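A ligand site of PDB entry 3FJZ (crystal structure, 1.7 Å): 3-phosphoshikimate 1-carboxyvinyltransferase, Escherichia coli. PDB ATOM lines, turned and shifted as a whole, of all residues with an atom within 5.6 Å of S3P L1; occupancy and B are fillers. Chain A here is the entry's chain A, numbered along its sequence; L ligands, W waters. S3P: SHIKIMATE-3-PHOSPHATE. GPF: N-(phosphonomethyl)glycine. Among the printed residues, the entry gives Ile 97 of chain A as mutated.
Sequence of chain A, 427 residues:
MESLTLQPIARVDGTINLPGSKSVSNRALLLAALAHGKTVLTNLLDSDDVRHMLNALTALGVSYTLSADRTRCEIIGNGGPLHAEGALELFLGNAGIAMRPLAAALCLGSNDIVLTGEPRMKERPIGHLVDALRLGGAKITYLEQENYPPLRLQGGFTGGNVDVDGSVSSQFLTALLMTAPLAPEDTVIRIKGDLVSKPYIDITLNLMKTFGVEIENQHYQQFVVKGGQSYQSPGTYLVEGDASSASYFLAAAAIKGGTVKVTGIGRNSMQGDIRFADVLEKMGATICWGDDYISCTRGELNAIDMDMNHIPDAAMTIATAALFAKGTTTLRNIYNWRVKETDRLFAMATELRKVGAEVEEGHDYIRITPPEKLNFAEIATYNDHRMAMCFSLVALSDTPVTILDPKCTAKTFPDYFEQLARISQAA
Merely in contact with S3P L1: Ile 97 (3.5 Å) and Tyr 200 (3.3 Å). Hydrophobic or aromatic side chains that line S3P L1: Ile 97 and Tyr 200. Along chain A the residues within 4 Å of S3P L1 span positions 22 to 340. The nearest printed residue that does not touch S3P L1 is Val 168 (4.01 Å).
The backbone carbonyl oxygen (O) of Ser 23 is in hydrogen-bond range of the guanidinium group (NH2) of Arg 27, at 3.0 Å. The side-chain hydroxyl (OG) of Ser 169 sits at hydrogen-bond distance from the backbone NH (N) of Gln 171, 3.0 Å away. The side-chain carboxylate (OD2) of Asp 313 lies within salt-bridge range of the side-chain amino group (NZ) of Lys 340. NH1 of Arg 27 lies within hydrogen-bond range of O of Tyr 200, 3.3 Å away. The guanidinium group of Arg 27 is in hydrogen-bond range of the side-chain hydroxyl of Thr 204 (2.9 Å). The side-chain amide oxygen of Asn 336 lies close to the backbone carbonyl oxygen of Val 168 (3.1 Å). The side-chain hydroxyl of Thr 204 lies within hydrogen-bond range of the backbone carbonyl oxygen of Tyr 200. The guanidinium group (NH2) of Arg 100 sits at hydrogen-bond distance from the side-chain amide oxygen (OE1) of Gln 171 (2.8 Å).
The backbone NH of Ser 170 is in hydrogen-bond range of an oxygen (O6) of S3P L1. The side-chain hydroxyl (OG) of Ser 170 is in hydrogen-bond range of an oxygen (O6) of S3P L1 (2.6 Å). The side-chain hydroxyl (OG) of Ser 197 lies within hydrogen-bond range of an oxygen (O7) of S3P L1 (2.6 Å). O5 of S3P L1 lies within hydrogen-bond range of OG of Ser 23, at 2.6 Å. OG of Ser 169 is in hydrogen-bond range of O8 of S3P L1 (2.7 Å). An oxygen (O3) of S3P L1 lies within hydrogen-bond range of the side-chain carboxylate of Asp 313. An oxygen (O4) of S3P L1 lies within salt-bridge range of the guanidinium group (NH1) of Arg 27. The side-chain amino group (NZ) of Lys 22 sits at hydrogen-bond distance from an oxygen (O3) of S3P L1 (2.7 Å). The side-chain amino group of Lys 340 lies within salt-bridge range of an oxygen (O7) of S3P L1, at 2.8 Å. The side-chain amide oxygen (OD1) of Asn 336 sits close to an oxygen (O7) of S3P L1 (2.9 Å). NE2 of Gln 171 lies within hydrogen-bond range of O1 of S3P L1. The side-chain amino group (NZ) of Lys 22 lies within salt-bridge range of an oxygen (O1) of GPF L2. NE2 of Gln 171 lies within hydrogen-bond range of O2 of GPF L2, at 2.8 Å. The guanidinium group (NH2) of Arg 100 lies within salt-bridge range of an oxygen (O2) of GPF L2, at 3.9 Å. O5 of GPF L2 is in salt-bridge range of NE of Arg 386, 2.5 Å away. O5 of GPF L2 is in salt-bridge range of NH2 of Arg 344. The side-chain carboxylate (OE2) of Glu 341 lies within salt-bridge range of a nitrogen (N1) of GPF L2.
Water W1 lies within hydrogen-bond range of O8 of S3P L1 (2.6 Å) and O of Val 168 (3.0 Å). Water W3 lies within hydrogen-bond range of O4 of S3P L1 (2.7 Å), OG1 of Thr 174 (2.7 Å), OG of Ser 170 (2.9 Å), NH1 of Arg 27 (3.4 Å) and N of Gln 171 (3.4 Å). Water W4 lies within hydrogen-bond range of O8 of S3P L1, NH2 of Arg 100, O2 of GPF L2 and NE2 of Gln 171. Water W2 lies within hydrogen-bond range of OG of Ser 23, NZ of Lys 22 and O3 of S3P L1.
An oxygen (O3) of S3P L1 is in hydrogen-bond range of a nitrogen (N1) of GPF L2, at 2.8 Å.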
ATOM      1  N   LYS A  22     -15.822  12.457 -11.691  1.00  0.00           N
ATOM      2  CA  LYS A  22     -16.605  11.310 -11.229  1.00  0.00           C
ATOM      3  C   LYS A  22     -16.982  11.497  -9.750  1.00  0.00           C
ATOM      4  O   LYS A  22     -18.127  11.264  -9.344  1.00  0.00           O
ATOM      5  CB  LYS A  22     -15.794  10.008 -11.410  1.00  0.00           C
ATOM      6  CG  LYS A  22     -16.485   8.745 -10.853  1.00  0.00           C
ATOM      7  CD  LYS A  22     -15.728   8.121  -9.650  1.00  0.00           C
ATOM      8  CE  LYS A  22     -14.412   7.473 -10.110  1.00  0.00           C
ATOM      9  NZ  LYS A  22     -13.513   7.102  -8.950  1.00  0.00           N
ATOM     10  N   SER A  23     -16.014  11.930  -8.952  1.00  0.00           N
ATOM     11  CA  SER A  23     -16.228  12.152  -7.509  1.00  0.00           C
ATOM     12  C   SER A  23     -17.324  13.177  -7.250  1.00  0.00           C
ATOM     13  O   SER A  23     -18.225  12.960  -6.426  1.00  0.00           O
ATOM     14  CB  SER A  23     -14.922  12.610  -6.853  1.00  0.00           C
ATOM     15  OG  SER A  23     -13.970  11.558  -6.876  1.00  0.00           O
ATOM     16  N   ARG A  27     -21.580  12.461  -6.093  1.00  0.00           N
ATOM     17  CA  ARG A  27     -22.027  13.088  -4.862  1.00  0.00           C
ATOM     18  C   ARG A  27     -23.184  14.048  -5.181  1.00  0.00           C
ATOM     19  O   ARG A  27     -24.199  14.083  -4.457  1.00  0.00           O
ATOM     20  CB  ARG A  27     -20.903  13.896  -4.227  1.00  0.00           C
ATOM     21  CG  ARG A  27     -19.873  13.040  -3.491  1.00  0.00           C
ATOM     22  CD  ARG A  27     -18.733  13.973  -3.116  1.00  0.00           C
ATOM     23  NE  ARG A  27     -17.713  13.376  -2.281  1.00  0.00           N
ATOM     24  CZ  ARG A  27     -16.761  12.528  -2.699  1.00  0.00           C
ATOM     25  NH1 ARG A  27     -15.863  12.070  -1.828  1.00  0.00           N
ATOM     26  NH2 ARG A  27     -16.726  12.119  -3.972  1.00  0.00           N
ATOM     27  N   ILE A  97     -17.802   4.961  -5.366  1.00  0.00           N
ATOM     28  CA  ILE A  97     -18.464   6.180  -4.929  1.00  0.00           C
ATOM     29  C   ILE A  97     -19.974   6.152  -5.176  1.00  0.00           C
ATOM     30  O   ILE A  97     -20.674   7.152  -4.954  1.00  0.00           O
ATOM     31  CB  ILE A  97     -17.741   7.460  -5.483  1.00  0.00           C
ATOM     32  CG1 ILE A  97     -18.048   8.685  -4.576  1.00  0.00           C
ATOM     33  CG2 ILE A  97     -18.143   7.694  -6.919  1.00  0.00           C
ATOM     34  CD1 ILE A  97     -17.564   8.546  -3.124  1.00  0.00           C
ATOM     35  N   ARG A 100     -20.470   2.871  -1.766  1.00  0.00           N
ATOM     36  CA  ARG A 100     -20.304   3.295  -0.395  1.00  0.00           C
ATOM     37  C   ARG A 100     -21.365   4.330   0.032  1.00  0.00           C
ATOM     38  O   ARG A 100     -22.058   4.122   1.022  1.00  0.00           O
ATOM     39  CB  ARG A 100     -18.861   3.785  -0.149  1.00  0.00           C
ATOM     40  CG  ARG A 100     -17.838   2.649   0.116  1.00  0.00           C
ATOM     41  CD  ARG A 100     -17.642   1.713  -1.107  1.00  0.00           C
ATOM     42  NE  ARG A 100     -16.574   0.716  -0.899  1.00  0.00           N
ATOM     43  CZ  ARG A 100     -15.280   0.935  -1.149  1.00  0.00           C
ATOM     44  NH1 ARG A 100     -14.391  -0.020  -0.943  1.00  0.00           N
ATOM     45  NH2 ARG A 100     -14.851   2.116  -1.642  1.00  0.00           N
ATOM     46  N   VAL A 168      -8.479   2.477   5.611  1.00  0.00           N
ATOM     47  CA  VAL A 168      -8.514   1.759   4.317  1.00  0.00           C
ATOM     48  C   VAL A 168      -9.178   2.572   3.214  1.00  0.00           C
ATOM     49  O   VAL A 168      -8.730   2.563   2.058  1.00  0.00           O
ATOM     50  CB  VAL A 168      -9.239   0.392   4.478  1.00  0.00           C
ATOM     51  CG1 VAL A 168      -9.386  -0.296   3.123  1.00  0.00           C
ATOM     52  CG2 VAL A 168      -8.441  -0.512   5.413  1.00  0.00           C
ATOM     53  N   SER A 169     -10.263   3.260   3.548  1.00  0.00           N
ATOM     54  CA  SER A 169     -10.954   4.108   2.569  1.00  0.00           C
ATOM     55  C   SER A 169     -11.592   5.326   3.207  1.00  0.00           C
ATOM     56  O   SER A 169     -12.225   5.224   4.266  1.00  0.00           O
ATOM     57  CB  SER A 169     -12.053   3.326   1.829  1.00  0.00           C
ATOM     58  OG  SER A 169     -12.686   4.174   0.861  1.00  0.00           O
ATOM     59  N   SER A 170     -11.422   6.472   2.568  1.00  0.00           N
ATOM     60  CA  SER A 170     -12.076   7.674   3.067  1.00  0.00           C
ATOM     61  C   SER A 170     -13.559   7.618   2.681  1.00  0.00           C
ATOM     62  O   SER A 170     -14.372   8.360   3.217  1.00  0.00           O
ATOM     63  CB  SER A 170     -11.484   8.934   2.425  1.00  0.00           C
ATOM     64  OG  SER A 170     -11.706   8.946   1.013  1.00  0.00           O
ATOM     65  N   GLN A 171     -13.913   6.746   1.740  1.00  0.00           N
ATOM     66  CA  GLN A 171     -15.294   6.664   1.299  1.00  0.00           C
ATOM     67  C   GLN A 171     -16.279   6.271   2.376  1.00  0.00           C
ATOM     68  O   GLN A 171     -17.458   6.622   2.302  1.00  0.00           O
ATOM     69  CB  GLN A 171     -15.430   5.710   0.129  1.00  0.00           C
ATOM     70  CG  GLN A 171     -14.802   6.279  -1.113  1.00  0.00           C
ATOM     71  CD  GLN A 171     -15.063   5.422  -2.321  1.00  0.00           C
ATOM     72  OE1 GLN A 171     -15.941   4.564  -2.312  1.00  0.00           O
ATOM     73  NE2 GLN A 171     -14.299   5.651  -3.385  1.00  0.00           N
ATOM     74  N   THR A 174     -16.996   9.472   4.122  1.00  0.00           N
ATOM     75  CA  THR A 174     -17.780  10.284   3.210  1.00  0.00           C
ATOM     76  C   THR A 174     -19.242   9.829   3.225  1.00  0.00           C
ATOM     77  O   THR A 174     -20.170  10.658   3.279  1.00  0.00           O
ATOM     78  CB  THR A 174     -17.217  10.161   1.776  1.00  0.00           C
ATOM     79  OG1 THR A 174     -16.194  11.152   1.646  1.00  0.00           O
ATOM     80  CG2 THR A 174     -18.320  10.371   0.702  1.00  0.00           C
ATOM     81  N   VAL A 196      -6.992   7.968   5.513  1.00  0.00           N
ATOM     82  CA  VAL A 196      -6.325   8.037   4.220  1.00  0.00           C
ATOM     83  C   VAL A 196      -7.195   8.825   3.249  1.00  0.00           C
ATOM     84  O   VAL A 196      -8.369   9.082   3.531  1.00  0.00           O
ATOM     85  CB  VAL A 196      -6.046   6.624   3.631  1.00  0.00           C
ATOM     86  CG1 VAL A 196      -5.048   5.874   4.509  1.00  0.00           C
ATOM     87  CG2 VAL A 196      -7.344   5.846   3.511  1.00  0.00           C
ATOM     88  N   SER A 197      -6.583   9.227   2.135  1.00  0.00           N
ATOM     89  CA  SER A 197      -7.279   9.974   1.075  1.00  0.00           C
ATOM     90  C   SER A 197      -8.059  11.134   1.645  1.00  0.00           C
ATOM     91  O   SER A 197      -9.191  11.435   1.223  1.00  0.00           O
ATOM     92  CB  SER A 197      -8.235   9.035   0.322  1.00  0.00           C
ATOM     93  OG  SER A 197      -7.490   8.057  -0.386  1.00  0.00           O
ATOM     94  N   TYR A 200     -10.476  13.821  -0.204  1.00  0.00           N
ATOM     95  CA  TYR A 200     -11.818  13.489  -0.668  1.00  0.00           C
ATOM     96  C   TYR A 200     -12.855  13.860   0.373  1.00  0.00           C
ATOM     97  O   TYR A 200     -14.018  14.102   0.024  1.00  0.00           O
ATOM     98  CB  TYR A 200     -11.900  12.008  -1.040  1.00  0.00           C
ATOM     99  CG  TYR A 200     -11.172  11.751  -2.331  1.00  0.00           C
ATOM    100  CD1 TYR A 200      -9.865  11.257  -2.329  1.00  0.00           C
ATOM    101  CD2 TYR A 200     -11.790  12.006  -3.557  1.00  0.00           C
ATOM    102  CE1 TYR A 200      -9.190  11.026  -3.527  1.00  0.00           C
ATOM    103  CE2 TYR A 200     -11.120  11.784  -4.757  1.00  0.00           C
ATOM    104  CZ  TYR A 200      -9.822  11.290  -4.727  1.00  0.00           C
ATOM    105  OH  TYR A 200      -9.162  11.033  -5.907  1.00  0.00           O
ATOM    106  N   ILE A 203     -13.964  17.220  -0.424  1.00  0.00           N
ATOM    107  CA  ILE A 203     -14.887  17.286  -1.544  1.00  0.00           C
ATOM    108  C   ILE A 203     -16.276  17.023  -0.988  1.00  0.00           C
ATOM    109  O   ILE A 203     -17.227  17.717  -1.333  1.00  0.00           O
ATOM    110  CB  ILE A 203     -14.578  16.208  -2.634  1.00  0.00           C
ATOM    111  CG1 ILE A 203     -13.208  16.489  -3.272  1.00  0.00           C
ATOM    112  CG2 ILE A 203     -15.666  16.220  -3.696  1.00  0.00           C
ATOM    113  CD1 ILE A 203     -12.834  15.471  -4.357  1.00  0.00           C
ATOM    114  N   THR A 204     -16.407  16.029  -0.117  1.00  0.00           N
ATOM    115  CA  THR A 204     -17.713  15.697   0.447  1.00  0.00           C
ATOM    116  C   THR A 204     -18.315  16.871   1.218  1.00  0.00           C
ATOM    117  O   THR A 204     -19.482  17.200   1.067  1.00  0.00           O
ATOM    118  CB  THR A 204     -17.598  14.472   1.342  1.00  0.00           C
ATOM    119  OG1 THR A 204     -17.116  13.387   0.534  1.00  0.00           O
ATOM    120  CG2 THR A 204     -18.955  14.087   1.950  1.00  0.00           C
ATOM    121  N   PRO A 312      -3.902   9.323  -4.378  1.00  0.00           N
ATOM    122  CA  PRO A 312      -3.757   7.926  -4.766  1.00  0.00           C
ATOM    123  C   PRO A 312      -4.064   7.561  -6.209  1.00  0.00           C
ATOM    124  O   PRO A 312      -3.385   6.713  -6.794  1.00  0.00           O
ATOM    125  CB  PRO A 312      -4.649   7.196  -3.765  1.00  0.00           C
ATOM    126  CG  PRO A 312      -5.751   8.198  -3.493  1.00  0.00           C
ATOM    127  CD  PRO A 312      -4.923   9.474  -3.317  1.00  0.00           C
ATOM    128  N   ASP A 313      -5.078   8.194  -6.782  1.00  0.00           N
ATOM    129  CA  ASP A 313      -5.478   7.887  -8.153  1.00  0.00           C
ATOM    130  C   ASP A 313      -4.531   8.493  -9.169  1.00  0.00           C
ATOM    131  O   ASP A 313      -3.978   7.787 -10.011  1.00  0.00           O
ATOM    132  CB  ASP A 313      -6.888   8.394  -8.423  1.00  0.00           C
ATOM    133  CG  ASP A 313      -7.953   7.651  -7.637  1.00  0.00           C
ATOM    134  OD1 ASP A 313      -9.119   8.025  -7.797  1.00  0.00           O
ATOM    135  OD2 ASP A 313      -7.629   6.705  -6.883  1.00  0.00           O
ATOM    136  N   ASN A 336      -3.793   1.388  -0.170  1.00  0.00           N
ATOM    137  CA  ASN A 336      -5.110   1.086  -0.716  1.00  0.00           C
ATOM    138  C   ASN A 336      -5.267   0.928  -2.219  1.00  0.00           C
ATOM    139  O   ASN A 336      -6.350   0.650  -2.710  1.00  0.00           O
ATOM    140  CB  ASN A 336      -6.226   1.955  -0.062  1.00  0.00           C
ATOM    141  CG  ASN A 336      -6.306   3.375  -0.579  1.00  0.00           C
ATOM    142  OD1 ASN A 336      -7.094   4.168  -0.028  1.00  0.00           O
ATOM    143  ND2 ASN A 336      -5.540   3.719  -1.601  1.00  0.00           N
ATOM    144  N   LYS A 340      -8.647  -1.402  -4.751  1.00  0.00           N
ATOM    145  CA  LYS A 340      -9.463  -0.649  -5.694  1.00  0.00           C
ATOM    146  C   LYS A 340      -9.904  -1.444  -6.914  1.00  0.00           C
ATOM    147  O   LYS A 340     -10.213  -2.624  -6.775  1.00  0.00           O
ATOM    148  CB  LYS A 340      -8.768   0.651  -6.035  1.00  0.00           C
ATOM    149  CG  LYS A 340      -8.937   1.609  -4.833  1.00  0.00           C
ATOM    150  CD  LYS A 340      -8.055   2.819  -4.884  1.00  0.00           C
ATOM    151  CE  LYS A 340      -8.394   3.707  -3.685  1.00  0.00           C
ATOM    152  NZ  LYS A 340      -7.510   4.880  -3.591  1.00  0.00           N
ATOM    153  N   GLU A 341      -9.951  -0.849  -8.107  1.00  0.00           N
ATOM    154  CA  GLU A 341     -10.444  -1.569  -9.279  1.00  0.00           C
ATOM    155  C   GLU A 341      -9.800  -2.921  -9.486  1.00  0.00           C
ATOM    156  O   GLU A 341     -10.416  -3.854  -9.997  1.00  0.00           O
ATOM    157  CB  GLU A 341     -10.333  -0.706 -10.541  1.00  0.00           C
ATOM    158  CG  GLU A 341     -11.444   0.377 -10.618  1.00  0.00           C
ATOM    159  CD  GLU A 341     -11.170   1.649  -9.822  1.00  0.00           C
ATOM    160  OE1 GLU A 341     -10.347   1.658  -8.858  1.00  0.00           O
ATOM    161  OE2 GLU A 341     -11.818   2.672 -10.159  1.00  0.00           O
ATOM    162  N   ARG A 344      -3.787  -2.650  -7.547  1.00  0.00           N
ATOM    163  CA  ARG A 344      -2.962  -1.802  -8.373  1.00  0.00           C
ATOM    164  C   ARG A 344      -1.476  -1.891  -8.123  1.00  0.00           C
ATOM    165  O   ARG A 344      -0.686  -1.598  -9.016  1.00  0.00           O
ATOM    166  CB  ARG A 344      -3.459  -0.358  -8.270  1.00  0.00           C
ATOM    167  CG  ARG A 344      -4.798  -0.178  -8.997  1.00  0.00           C
ATOM    168  CD  ARG A 344      -5.420   1.164  -8.678  1.00  0.00           C
ATOM    169  NE  ARG A 344      -6.402   1.494  -9.716  1.00  0.00           N
ATOM    170  CZ  ARG A 344      -7.188   2.559  -9.674  1.00  0.00           C
ATOM    171  NH1 ARG A 344      -8.049   2.800 -10.675  1.00  0.00           N
ATOM    172  NH2 ARG A 344      -7.112   3.384  -8.632  1.00  0.00           N
ATOM    173  N   ARG A 386      -7.685   3.002 -15.122  1.00  0.00           N
ATOM    174  CA  ARG A 386      -6.404   3.679 -14.996  1.00  0.00           C
ATOM    175  C   ARG A 386      -5.212   2.886 -15.492  1.00  0.00           C
ATOM    176  O   ARG A 386      -4.194   3.479 -15.841  1.00  0.00           O
ATOM    177  CB  ARG A 386      -6.197   4.185 -13.563  1.00  0.00           C
ATOM    178  CG  ARG A 386      -7.295   5.174 -13.146  1.00  0.00           C
ATOM    179  CD  ARG A 386      -6.845   6.177 -12.058  1.00  0.00           C
ATOM    180  NE  ARG A 386      -8.057   6.861 -11.587  1.00  0.00           N
ATOM    181  CZ  ARG A 386      -8.711   7.809 -12.251  1.00  0.00           C
ATOM    182  NH1 ARG A 386      -9.844   8.294 -11.725  1.00  0.00           N
ATOM    183  NH2 ARG A 386      -8.217   8.330 -13.380  1.00  0.00           N
HETATM  184  C1  S3P L   1     -12.996   8.848  -4.086  1.00  0.00           C
HETATM  185  C2  S3P L   1     -12.068   8.532  -3.068  1.00  0.00           C
HETATM  186  C3  S3P L   1     -10.886   7.622  -3.332  1.00  0.00           C
HETATM  187  C4  S3P L   1     -10.582   7.490  -4.852  1.00  0.00           C
HETATM  188  C5  S3P L   1     -11.853   7.224  -5.668  1.00  0.00           C
HETATM  189  C6  S3P L   1     -12.843   8.371  -5.437  1.00  0.00           C
HETATM  190  C7  S3P L   1     -14.155   9.753  -3.747  1.00  0.00           C
HETATM  191  O1  S3P L   1     -11.062   6.312  -2.629  1.00  0.00           O
HETATM  192  O2  S3P L   1      -9.595   6.471  -5.022  1.00  0.00           O
HETATM  193  O3  S3P L   1     -11.539   7.137  -7.060  1.00  0.00           O
HETATM  194  O4  S3P L   1     -14.423   9.917  -2.537  1.00  0.00           O
HETATM  195  O5  S3P L   1     -14.688  10.341  -4.664  1.00  0.00           O
HETATM  196  P1  S3P L   1     -10.297   5.864  -1.168  1.00  0.00           P
HETATM  197  O6  S3P L   1     -10.768   6.760  -0.081  1.00  0.00           O
HETATM  198  O7  S3P L   1      -8.816   6.029  -1.391  1.00  0.00           O
HETATM  199  O8  S3P L   1     -10.688   4.474  -0.879  1.00  0.00           O
HETATM  200  C1  GPF L   2     -12.188   3.570  -6.820  1.00  0.00           C
HETATM  201  C2  GPF L   2     -10.245   4.492  -8.122  1.00  0.00           C
HETATM  202  C3  GPF L   2      -9.962   5.393  -9.320  1.00  0.00           C
HETATM  203  O1  GPF L   2     -14.292   5.093  -7.134  1.00  0.00           O
HETATM  204  O2  GPF L   2     -14.111   3.508  -5.182  1.00  0.00           O
HETATM  205  O3  GPF L   2     -14.562   2.673  -7.515  1.00  0.00           O
HETATM  206  O4  GPF L   2     -10.942   6.003  -9.873  1.00  0.00           O
HETATM  207  P1  GPF L   2     -13.901   3.742  -6.650  1.00  0.00           P
HETATM  208  O5  GPF L   2      -8.791   5.476  -9.681  1.00  0.00           O
HETATM  209  N1  GPF L   2     -11.673   4.474  -7.835  1.00  0.00           N
HETATM  210  O   HOH W   1      -9.897   1.974  -0.660  1.00  0.00           O
HETATM  211  O   HOH W   2     -12.632   9.931  -8.795  1.00  0.00           O
HETATM  212  O   HOH W   3     -14.305   9.787   0.189  1.00  0.00           O
HETATM  213  O   HOH W   4     -12.250   3.162  -2.794  1.00  0.00           O
